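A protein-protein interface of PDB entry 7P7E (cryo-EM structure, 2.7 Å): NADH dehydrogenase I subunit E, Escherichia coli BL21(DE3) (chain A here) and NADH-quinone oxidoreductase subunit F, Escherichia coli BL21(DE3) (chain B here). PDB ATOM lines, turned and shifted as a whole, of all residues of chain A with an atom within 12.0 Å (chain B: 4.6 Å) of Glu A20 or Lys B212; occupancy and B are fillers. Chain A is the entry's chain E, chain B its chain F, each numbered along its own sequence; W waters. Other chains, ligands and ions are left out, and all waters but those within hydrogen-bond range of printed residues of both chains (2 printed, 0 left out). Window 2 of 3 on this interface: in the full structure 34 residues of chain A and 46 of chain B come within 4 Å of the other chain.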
ATOM      1  N   ILE A  12      33.614   5.857  19.914  1.00  0.00           N
ATOM      2  CA  ILE A  12      32.952   4.726  19.271  1.00  0.00           C
ATOM      3  C   ILE A  12      31.441   4.807  19.455  1.00  0.00           C
ATOM      4  O   ILE A  12      30.680   4.609  18.502  1.00  0.00           O
ATOM      5  CB  ILE A  12      33.528   3.402  19.804  1.00  0.00           C
ATOM      6  CG1 ILE A  12      34.914   3.150  19.214  1.00  0.00           C
ATOM      7  CG2 ILE A  12      32.622   2.238  19.466  1.00  0.00           C
ATOM      8  CD1 ILE A  12      35.696   2.077  19.928  1.00  0.00           C
ATOM      9  N   GLU A  13      30.978   5.137  20.665  1.00  0.00           N
ATOM     10  CA  GLU A  13      29.538   5.240  20.897  1.00  0.00           C
ATOM     11  C   GLU A  13      28.933   6.431  20.160  1.00  0.00           C
ATOM     12  O   GLU A  13      27.801   6.351  19.657  1.00  0.00           O
ATOM     13  CB  GLU A  13      29.257   5.328  22.396  1.00  0.00           C
ATOM     14  CG  GLU A  13      29.092   3.971  23.060  1.00  0.00           C
ATOM     15  CD  GLU A  13      29.782   3.890  24.406  1.00  0.00           C
ATOM     16  OE1 GLU A  13      30.432   4.877  24.805  1.00  0.00           O
ATOM     17  OE2 GLU A  13      29.675   2.833  25.065  1.00  0.00           O
ATOM     18  N   HIS A  14      29.679   7.538  20.069  1.00  0.00           N
ATOM     19  CA  HIS A  14      29.209   8.688  19.306  1.00  0.00           C
ATOM     20  C   HIS A  14      29.080   8.349  17.828  1.00  0.00           C
ATOM     21  O   HIS A  14      28.159   8.823  17.152  1.00  0.00           O
ATOM     22  CB  HIS A  14      30.151   9.873  19.503  1.00  0.00           C
ATOM     23  CG  HIS A  14      29.746  11.095  18.741  1.00  0.00           C
ATOM     24  ND1 HIS A  14      28.577  11.777  18.997  1.00  0.00           N
ATOM     25  CD2 HIS A  14      30.351  11.755  17.726  1.00  0.00           C
ATOM     26  CE1 HIS A  14      28.480  12.806  18.176  1.00  0.00           C
ATOM     27  NE2 HIS A  14      29.544  12.815  17.393  1.00  0.00           N
ATOM     28  N   GLU A  15      29.995   7.531  17.306  1.00  0.00           N
ATOM     29  CA  GLU A  15      29.849   7.057  15.935  1.00  0.00           C
ATOM     30  C   GLU A  15      28.706   6.058  15.803  1.00  0.00           C
ATOM     31  O   GLU A  15      28.082   5.970  14.741  1.00  0.00           O
ATOM     32  CB  GLU A  15      31.160   6.445  15.457  1.00  0.00           C
ATOM     33  CG  GLU A  15      32.178   7.489  15.060  1.00  0.00           C
ATOM     34  CD  GLU A  15      31.820   8.176  13.759  1.00  0.00           C
ATOM     35  OE1 GLU A  15      31.342   7.487  12.833  1.00  0.00           O
ATOM     36  OE2 GLU A  15      32.013   9.407  13.661  1.00  0.00           O
ATOM     37  N   MET A  16      28.426   5.296  16.863  1.00  0.00           N
ATOM     38  CA  MET A  16      27.290   4.380  16.853  1.00  0.00           C
ATOM     39  C   MET A  16      25.962   5.121  16.804  1.00  0.00           C
ATOM     40  O   MET A  16      24.971   4.572  16.310  1.00  0.00           O
ATOM     41  CB  MET A  16      27.331   3.465  18.077  1.00  0.00           C
ATOM     42  CG  MET A  16      28.398   2.391  18.030  1.00  0.00           C
ATOM     43  SD  MET A  16      28.623   1.575  19.622  1.00  0.00           S
ATOM     44  CE  MET A  16      27.081   0.683  19.777  1.00  0.00           C
ATOM     45  N   HIS A  17      25.913   6.355  17.318  1.00  0.00           N
ATOM     46  CA  HIS A  17      24.674   7.129  17.233  1.00  0.00           C
ATOM     47  C   HIS A  17      24.302   7.519  15.804  1.00  0.00           C
ATOM     48  O   HIS A  17      23.131   7.817  15.549  1.00  0.00           O
ATOM     49  CB  HIS A  17      24.764   8.400  18.083  1.00  0.00           C
ATOM     50  CG  HIS A  17      25.103   8.151  19.518  1.00  0.00           C
ATOM     51  ND1 HIS A  17      25.969   8.954  20.228  1.00  0.00           N
ATOM     52  CD2 HIS A  17      24.691   7.190  20.380  1.00  0.00           C
ATOM     53  CE1 HIS A  17      26.077   8.499  21.463  1.00  0.00           C
ATOM     54  NE2 HIS A  17      25.312   7.429  21.581  1.00  0.00           N
ATOM     55  N   HIS A  18      25.253   7.524  14.872  1.00  0.00           N
ATOM     56  CA  HIS A  18      25.006   8.042  13.530  1.00  0.00           C
ATOM     57  C   HIS A  18      24.394   7.023  12.577  1.00  0.00           C
ATOM     58  O   HIS A  18      24.105   7.379  11.431  1.00  0.00           O
ATOM     59  CB  HIS A  18      26.306   8.569  12.916  1.00  0.00           C
ATOM     60  CG  HIS A  18      26.968   9.640  13.724  1.00  0.00           C
ATOM     61  ND1 HIS A  18      28.331   9.687  13.920  1.00  0.00           N
ATOM     62  CD2 HIS A  18      26.454  10.703  14.387  1.00  0.00           C
ATOM     63  CE1 HIS A  18      28.629  10.734  14.668  1.00  0.00           C
ATOM     64  NE2 HIS A  18      27.508  11.368  14.964  1.00  0.00           N
ATOM     65  N   TYR A  19      24.188   5.779  13.001  1.00  0.00           N
ATOM     66  CA  TYR A  19      23.735   4.734  12.098  1.00  0.00           C
ATOM     67  C   TYR A  19      22.530   4.005  12.670  1.00  0.00           C
ATOM     68  O   TYR A  19      22.319   3.971  13.885  1.00  0.00           O
ATOM     69  CB  TYR A  19      24.846   3.722  11.810  1.00  0.00           C
ATOM     70  CG  TYR A  19      26.098   4.333  11.234  1.00  0.00           C
ATOM     71  CD1 TYR A  19      26.157   4.715   9.901  1.00  0.00           C
ATOM     72  CD2 TYR A  19      27.224   4.519  12.021  1.00  0.00           C
ATOM     73  CE1 TYR A  19      27.302   5.270   9.371  1.00  0.00           C
ATOM     74  CE2 TYR A  19      28.373   5.074  11.500  1.00  0.00           C
ATOM     75  CZ  TYR A  19      28.406   5.447  10.175  1.00  0.00           C
ATOM     76  OH  TYR A  19      29.551   6.001   9.653  1.00  0.00           O
ATOM     77  N   GLU A  20      21.737   3.431  11.765  1.00  0.00           N
ATOM     78  CA  GLU A  20      20.611   2.591  12.160  1.00  0.00           C
ATOM     79  C   GLU A  20      21.086   1.323  12.862  1.00  0.00           C
ATOM     80  O   GLU A  20      20.503   0.906  13.869  1.00  0.00           O
ATOM     81  CB  GLU A  20      19.773   2.259  10.924  1.00  0.00           C
ATOM     82  CG  GLU A  20      19.059   0.922  10.953  1.00  0.00           C
ATOM     83  CD  GLU A  20      18.180   0.714   9.739  1.00  0.00           C
ATOM     84  OE1 GLU A  20      17.976   1.683   8.979  1.00  0.00           O
ATOM     85  OE2 GLU A  20      17.691  -0.419   9.542  1.00  0.00           O
ATOM     86  N   ASP A  21      22.151   0.710  12.355  1.00  0.00           N
ATOM     87  CA  ASP A  21      22.725  -0.511  12.889  1.00  0.00           C
ATOM     88  C   ASP A  21      24.059  -0.186  13.541  1.00  0.00           C
ATOM     89  O   ASP A  21      24.898   0.471  12.911  1.00  0.00           O
ATOM     90  CB  ASP A  21      22.915  -1.533  11.753  1.00  0.00           C
ATOM     91  CG  ASP A  21      23.187  -2.954  12.244  1.00  0.00           C
ATOM     92  OD1 ASP A  21      23.638  -3.162  13.386  1.00  0.00           O
ATOM     93  OD2 ASP A  21      22.954  -3.889  11.452  1.00  0.00           O
ATOM     94  N   PRO A  22      24.285  -0.595  14.794  1.00  0.00           N
ATOM     95  CA  PRO A  22      25.591  -0.347  15.429  1.00  0.00           C
ATOM     96  C   PRO A  22      26.763  -1.044  14.756  1.00  0.00           C
ATOM     97  O   PRO A  22      27.908  -0.659  15.012  1.00  0.00           O
ATOM     98  CB  PRO A  22      25.388  -0.861  16.862  1.00  0.00           C
ATOM     99  CG  PRO A  22      24.155  -1.701  16.812  1.00  0.00           C
ATOM    100  CD  PRO A  22      23.295  -1.072  15.771  1.00  0.00           C
ATOM    101  N   ARG A  23      26.518  -2.058  13.920  1.00  0.00           N
ATOM    102  CA  ARG A  23      27.597  -2.713  13.183  1.00  0.00           C
ATOM    103  C   ARG A  23      28.283  -1.756  12.215  1.00  0.00           C
ATOM    104  O   ARG A  23      29.473  -1.914  11.923  1.00  0.00           O
ATOM    105  CB  ARG A  23      27.041  -3.928  12.436  1.00  0.00           C
ATOM    106  CG  ARG A  23      28.068  -4.741  11.663  1.00  0.00           C
ATOM    107  CD  ARG A  23      27.409  -5.579  10.588  1.00  0.00           C
ATOM    108  NE  ARG A  23      26.634  -6.670  11.163  1.00  0.00           N
ATOM    109  CZ  ARG A  23      27.145  -7.833  11.536  1.00  0.00           C
ATOM    110  NH1 ARG A  23      28.432  -8.101  11.390  1.00  0.00           N
ATOM    111  NH2 ARG A  23      26.347  -8.750  12.072  1.00  0.00           N
ATOM    112  N   ALA A  24      27.567  -0.731  11.748  1.00  0.00           N
ATOM    113  CA  ALA A  24      28.089   0.203  10.760  1.00  0.00           C
ATOM    114  C   ALA A  24      29.217   1.080  11.285  1.00  0.00           C
ATOM    115  O   ALA A  24      29.868   1.762  10.487  1.00  0.00           O
ATOM    116  CB  ALA A  24      26.954   1.080  10.235  1.00  0.00           C
ATOM    117  N   ALA A  25      29.467   1.086  12.591  1.00  0.00           N
ATOM    118  CA  ALA A  25      30.544   1.864  13.181  1.00  0.00           C
ATOM    119  C   ALA A  25      31.838   1.074  13.340  1.00  0.00           C
ATOM    120  O   ALA A  25      32.767   1.569  13.979  1.00  0.00           O
ATOM    121  CB  ALA A  25      30.109   2.416  14.539  1.00  0.00           C
ATOM    122  N   SER A  26      31.917  -0.137  12.777  1.00  0.00           N
ATOM    123  CA  SER A  26      33.086  -0.992  12.985  1.00  0.00           C
ATOM    124  C   SER A  26      34.335  -0.425  12.322  1.00  0.00           C
ATOM    125  O   SER A  26      35.421  -0.447  12.917  1.00  0.00           O
ATOM    126  CB  SER A  26      32.799  -2.401  12.469  1.00  0.00           C
ATOM    127  OG  SER A  26      32.621  -2.409  11.064  1.00  0.00           O
ATOM    128  N   LEU A  52      30.507  -3.080  20.228  1.00  0.00           N
ATOM    129  CA  LEU A  52      29.544  -2.959  19.141  1.00  0.00           C
ATOM    130  C   LEU A  52      28.453  -4.021  19.166  1.00  0.00           C
ATOM    131  O   LEU A  52      27.460  -3.875  18.447  1.00  0.00           O
ATOM    132  CB  LEU A  52      30.267  -3.019  17.798  1.00  0.00           C
ATOM    133  CG  LEU A  52      30.479  -1.688  17.090  1.00  0.00           C
ATOM    134  CD1 LEU A  52      31.577  -0.897  17.760  1.00  0.00           C
ATOM    135  CD2 LEU A  52      30.827  -1.961  15.654  1.00  0.00           C
ATOM    136  N   GLY A  53      28.605  -5.078  19.957  1.00  0.00           N
ATOM    137  CA  GLY A  53      27.612  -6.131  19.977  1.00  0.00           C
ATOM    138  C   GLY A  53      27.652  -7.071  18.797  1.00  0.00           C
ATOM    139  O   GLY A  53      26.655  -7.745  18.523  1.00  0.00           O
ATOM    140  N   ILE A  54      28.769  -7.139  18.088  1.00  0.00           N
ATOM    141  CA  ILE A  54      28.919  -8.027  16.938  1.00  0.00           C
ATOM    142  C   ILE A  54      30.037  -9.006  17.265  1.00  0.00           C
ATOM    143  O   ILE A  54      30.863  -8.744  18.154  1.00  0.00           O
ATOM    144  CB  ILE A  54      29.183  -7.236  15.636  1.00  0.00           C
ATOM    145  CG1 ILE A  54      30.470  -6.420  15.740  1.00  0.00           C
ATOM    146  CG2 ILE A  54      28.001  -6.336  15.315  1.00  0.00           C
ATOM    147  CD1 ILE A  54      30.742  -5.567  14.521  1.00  0.00           C
ATOM    148  N   ILE B  84      12.161   5.217   5.150  1.00  0.00           N
ATOM    149  CA  ILE B  84      13.476   5.274   5.781  1.00  0.00           C
ATOM    150  C   ILE B  84      14.519   5.299   4.670  1.00  0.00           C
ATOM    151  O   ILE B  84      15.587   4.687   4.782  1.00  0.00           O
ATOM    152  CB  ILE B  84      13.696   4.097   6.754  1.00  0.00           C
ATOM    153  CG1 ILE B  84      12.385   3.703   7.437  1.00  0.00           C
ATOM    154  CG2 ILE B  84      14.717   4.459   7.830  1.00  0.00           C
ATOM    155  CD1 ILE B  84      11.897   4.700   8.475  1.00  0.00           C
ATOM    156  N   TYR B  86      17.400   6.381   1.929  1.00  0.00           N
ATOM    157  CA  TYR B  86      18.754   6.872   2.146  1.00  0.00           C
ATOM    158  C   TYR B  86      19.351   7.409   0.855  1.00  0.00           C
ATOM    159  O   TYR B  86      19.109   6.869  -0.233  1.00  0.00           O
ATOM    160  CB  TYR B  86      19.663   5.768   2.689  1.00  0.00           C
ATOM    161  CG  TYR B  86      19.395   5.396   4.123  1.00  0.00           C
ATOM    162  CD1 TYR B  86      19.794   6.223   5.160  1.00  0.00           C
ATOM    163  CD2 TYR B  86      18.746   4.212   4.440  1.00  0.00           C
ATOM    164  CE1 TYR B  86      19.551   5.884   6.474  1.00  0.00           C
ATOM    165  CE2 TYR B  86      18.500   3.864   5.750  1.00  0.00           C
ATOM    166  CZ  TYR B  86      18.904   4.704   6.761  1.00  0.00           C
ATOM    167  OH  TYR B  86      18.659   4.360   8.068  1.00  0.00           O
ATOM    168  N   ARG B 127      18.118  10.772   5.414  1.00  0.00           N
ATOM    169  CA  ARG B 127      19.520  10.708   5.792  1.00  0.00           C
ATOM    170  C   ARG B 127      20.403  10.628   4.558  1.00  0.00           C
ATOM    171  O   ARG B 127      20.073   9.946   3.579  1.00  0.00           O
ATOM    172  CB  ARG B 127      19.796   9.512   6.706  1.00  0.00           C
ATOM    173  CG  ARG B 127      19.769   9.868   8.173  1.00  0.00           C
ATOM    174  CD  ARG B 127      20.224   8.726   9.048  1.00  0.00           C
ATOM    175  NE  ARG B 127      20.186   9.097  10.456  1.00  0.00           N
ATOM    176  CZ  ARG B 127      20.292   8.240  11.460  1.00  0.00           C
ATOM    177  NH1 ARG B 127      20.441   6.943  11.250  1.00  0.00           N
ATOM    178  NH2 ARG B 127      20.244   8.696  12.709  1.00  0.00           N
ATOM    179  N   PRO B 204      19.332  -1.396  -5.351  1.00  0.00           N
ATOM    180  CA  PRO B 204      19.296  -0.623  -4.097  1.00  0.00           C
ATOM    181  C   PRO B 204      18.113   0.318  -3.974  1.00  0.00           C
ATOM    182  O   PRO B 204      17.801   0.745  -2.856  1.00  0.00           O
ATOM    183  CB  PRO B 204      20.616   0.153  -4.129  1.00  0.00           C
ATOM    184  CG  PRO B 204      21.510  -0.672  -4.959  1.00  0.00           C
ATOM    185  CD  PRO B 204      20.644  -1.283  -6.013  1.00  0.00           C
ATOM    186  N   THR B 206      15.044  -0.415  -4.246  1.00  0.00           N
ATOM    187  CA  THR B 206      14.016  -1.107  -3.479  1.00  0.00           C
ATOM    188  C   THR B 206      14.517  -1.620  -2.136  1.00  0.00           C
ATOM    189  O   THR B 206      13.804  -1.509  -1.135  1.00  0.00           O
ATOM    190  CB  THR B 206      13.441  -2.276  -4.287  1.00  0.00           C
ATOM    191  OG1 THR B 206      14.491  -3.182  -4.640  1.00  0.00           O
ATOM    192  CG2 THR B 206      12.772  -1.768  -5.548  1.00  0.00           C
ATOM    193  N   SER B 207      15.728  -2.175  -2.084  1.00  0.00           N
ATOM    194  CA  SER B 207      16.297  -2.659  -0.826  1.00  0.00           C
ATOM    195  C   SER B 207      17.807  -2.449  -0.889  1.00  0.00           C
ATOM    196  O   SER B 207      18.530  -3.285  -1.437  1.00  0.00           O
ATOM    197  CB  SER B 207      15.942  -4.120  -0.585  1.00  0.00           C
ATOM    198  OG  SER B 207      16.364  -4.935  -1.663  1.00  0.00           O
ATOM    199  N   GLY B 208      18.269  -1.337  -0.327  1.00  0.00           N
ATOM    200  CA  GLY B 208      19.675  -0.991  -0.371  1.00  0.00           C
ATOM    201  C   GLY B 208      20.338  -0.975   0.988  1.00  0.00           C
ATOM    202  O   GLY B 208      20.622  -2.031   1.558  1.00  0.00           O
ATOM    203  N   ALA B 209      20.593   0.222   1.511  1.00  0.00           N
ATOM    204  CA  ALA B 209      21.263   0.365   2.797  1.00  0.00           C
ATOM    205  C   ALA B 209      20.327  -0.052   3.922  1.00  0.00           C
ATOM    206  O   ALA B 209      19.261   0.546   4.103  1.00  0.00           O
ATOM    207  CB  ALA B 209      21.735   1.802   2.991  1.00  0.00           C
ATOM    208  N   TRP B 210      20.734  -1.087   4.666  1.00  0.00           N
ATOM    209  CA  TRP B 210      19.966  -1.672   5.769  1.00  0.00           C
ATOM    210  C   TRP B 210      18.581  -2.132   5.324  1.00  0.00           C
ATOM    211  O   TRP B 210      17.620  -2.075   6.093  1.00  0.00           O
ATOM    212  CB  TRP B 210      19.862  -0.704   6.954  1.00  0.00           C
ATOM    213  CG  TRP B 210      21.196  -0.299   7.501  1.00  0.00           C
ATOM    214  CD1 TRP B 210      22.012  -1.043   8.296  1.00  0.00           C
ATOM    215  CD2 TRP B 210      21.871   0.945   7.286  1.00  0.00           C
ATOM    216  NE1 TRP B 210      23.152  -0.341   8.593  1.00  0.00           N
ATOM    217  CE2 TRP B 210      23.090   0.884   7.985  1.00  0.00           C
ATOM    218  CE3 TRP B 210      21.560   2.106   6.574  1.00  0.00           C
ATOM    219  CZ2 TRP B 210      23.999   1.936   7.991  1.00  0.00           C
ATOM    220  CZ3 TRP B 210      22.465   3.149   6.581  1.00  0.00           C
ATOM    221  CH2 TRP B 210      23.669   3.058   7.284  1.00  0.00           C
ATOM    222  N   GLY B 211      18.468  -2.589   4.080  1.00  0.00           N
ATOM    223  CA  GLY B 211      17.214  -3.070   3.543  1.00  0.00           C
ATOM    224  C   GLY B 211      16.241  -1.999   3.107  1.00  0.00           C
ATOM    225  O   GLY B 211      15.143  -2.338   2.651  1.00  0.00           O
ATOM    226  N   LYS B 212      16.600  -0.733   3.227  1.00  0.00           N
ATOM    227  CA  LYS B 212      15.729   0.377   2.883  1.00  0.00           C
ATOM    228  C   LYS B 212      15.988   0.837   1.457  1.00  0.00           C
ATOM    229  O   LYS B 212      17.022   0.506   0.871  1.00  0.00           O
ATOM    230  CB  LYS B 212      15.951   1.532   3.856  1.00  0.00           C
ATOM    231  CG  LYS B 212      15.846   1.136   5.315  1.00  0.00           C
ATOM    232  CD  LYS B 212      14.486   0.548   5.629  1.00  0.00           C
ATOM    233  CE  LYS B 212      14.353   0.239   7.106  1.00  0.00           C
ATOM    234  NZ  LYS B 212      15.316  -0.810   7.539  1.00  0.00           N
ATOM    235  N   PRO B 213      15.038   1.549   0.850  1.00  0.00           N
ATOM    236  CA  PRO B 213      15.312   2.204  -0.436  1.00  0.00           C
ATOM    237  C   PRO B 213      16.492   3.158  -0.329  1.00  0.00           C
ATOM    238  O   PRO B 213      16.600   3.941   0.615  1.00  0.00           O
ATOM    239  CB  PRO B 213      14.006   2.946  -0.746  1.00  0.00           C
ATOM    240  CG  PRO B 213      13.048   2.603   0.357  1.00  0.00           C
ATOM    241  CD  PRO B 213      13.596   1.460   1.116  1.00  0.00           C
ATOM    242  N   THR B 214      17.386   3.081  -1.310  1.00  0.00           N
ATOM    243  CA  THR B 214      18.679   3.745  -1.224  1.00  0.00           C
ATOM    244  C   THR B 214      19.111   4.148  -2.623  1.00  0.00           C
ATOM    245  O   THR B 214      19.003   3.348  -3.557  1.00  0.00           O
ATOM    246  CB  THR B 214      19.722   2.816  -0.585  1.00  0.00           C
ATOM    247  OG1 THR B 214      19.343   2.526   0.766  1.00  0.00           O
ATOM    248  CG2 THR B 214      21.097   3.448  -0.582  1.00  0.00           C
HETATM  249  O   HOH W   1      25.273  -2.327   9.600  1.00  0.00           O
HETATM  250  O   HOH W   2      21.417   4.852   9.306  1.00  0.00           O
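OE2 of Glu A20 is in salt-bridge range of NZ of Lys B212.
The side-chain hydroxyl (OH) of Tyr B86 is in hydrogen-bond range of the side-chain carboxylate (OE1) of Glu A20 (2.9 Å).
The backbone carbonyl oxygen of Lys B212 sits at hydrogen-bond distance from the side-chain hydroxyl of Thr B214, at 3.1 Å.
OD1 of Asp A21 lies close to N of Arg A23, at 3.1 Å.
O of His A14 lies close to ND1 of His A18, 3.3 Å away.
The backbone carbonyl oxygen (O) of Pro B213 lies within hydrogen-bond range of the backbone NH (N) of Tyr B86 (2.9 Å).
NZ of Lys B212 sits at hydrogen-bond distance from O of Trp B210 (3.0 Å).
His A18 touches Arg B127 (O to NH1, 3.7 Å).
Arg B127 touches Tyr A19 (NH1 to C, 3.9 Å).
CD1 of Tyr A19 touches CH2 of Trp B210, 3.97 Å away.
NH1 of Arg B127 touches N of Glu A20, 3.8 Å away.
Glu A20 touches Trp B210.
Asp A21 touches Trp B210.
CB of Ala A24 touches CZ2 of Trp B210 (3.8 Å).
Of chain B, only Tyr B86, Arg B127, Trp B210 and Lys B212 come within 4 Å of Glu A20.
No residue of chain A comes within 4 Å of Ile B84.
Of the printed residues of chain A, Tyr B86 touches Glu A20.
No residue of chain A comes within 4 Å of Ala B209.
Trp B210 touches four residues of chain A.
No residue of chain A comes within 4 Å of Pro B213.
Of the printed residues of chain B, His A18 touches Arg B127 (3.7 Å).
Printed residues of chain B within 4 Å of Asp A21: Trp B210 (3.4 Å).
Printed residues of chain B within 4 Å of Ala A24: Trp B210.
The nearest printed residue of chain B that does not touch Asp A21 is Arg B127 (6.6 Å).
Of the 13 printed residues of chain B, 4 touch a printed residue of chain A.
Hydrophobic or aromatic side chains of chain B within 4 Å of the printed part of chain A: Tyr B86 and Trp B210.
Of the 18 printed residues of chain A, 5 touch a printed residue of chain B.
Printed residues of chain A that touch a printed residue of chain B: His A18, Tyr A19, Glu A20, Asp A21 and Ala A24.
Among the printed residues, Asp or Glu carboxylates within 4 Å of a Lys or Arg side-chain nitrogen of the other chain: Glu A20 with Lys B212.
Water W2 lies within hydrogen-bond range of the backbone NH (N) of Glu A20 (2.9 Å), the guanidinium group (NH1) of Arg B127 (3.0 Å) and the side-chain hydroxyl (OH) of Tyr B86 (3.1 Å).
Water W1 bridges the indole nitrogen (NE1) of Trp B210 and the side-chain carboxylate (OD2) of Asp A21.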
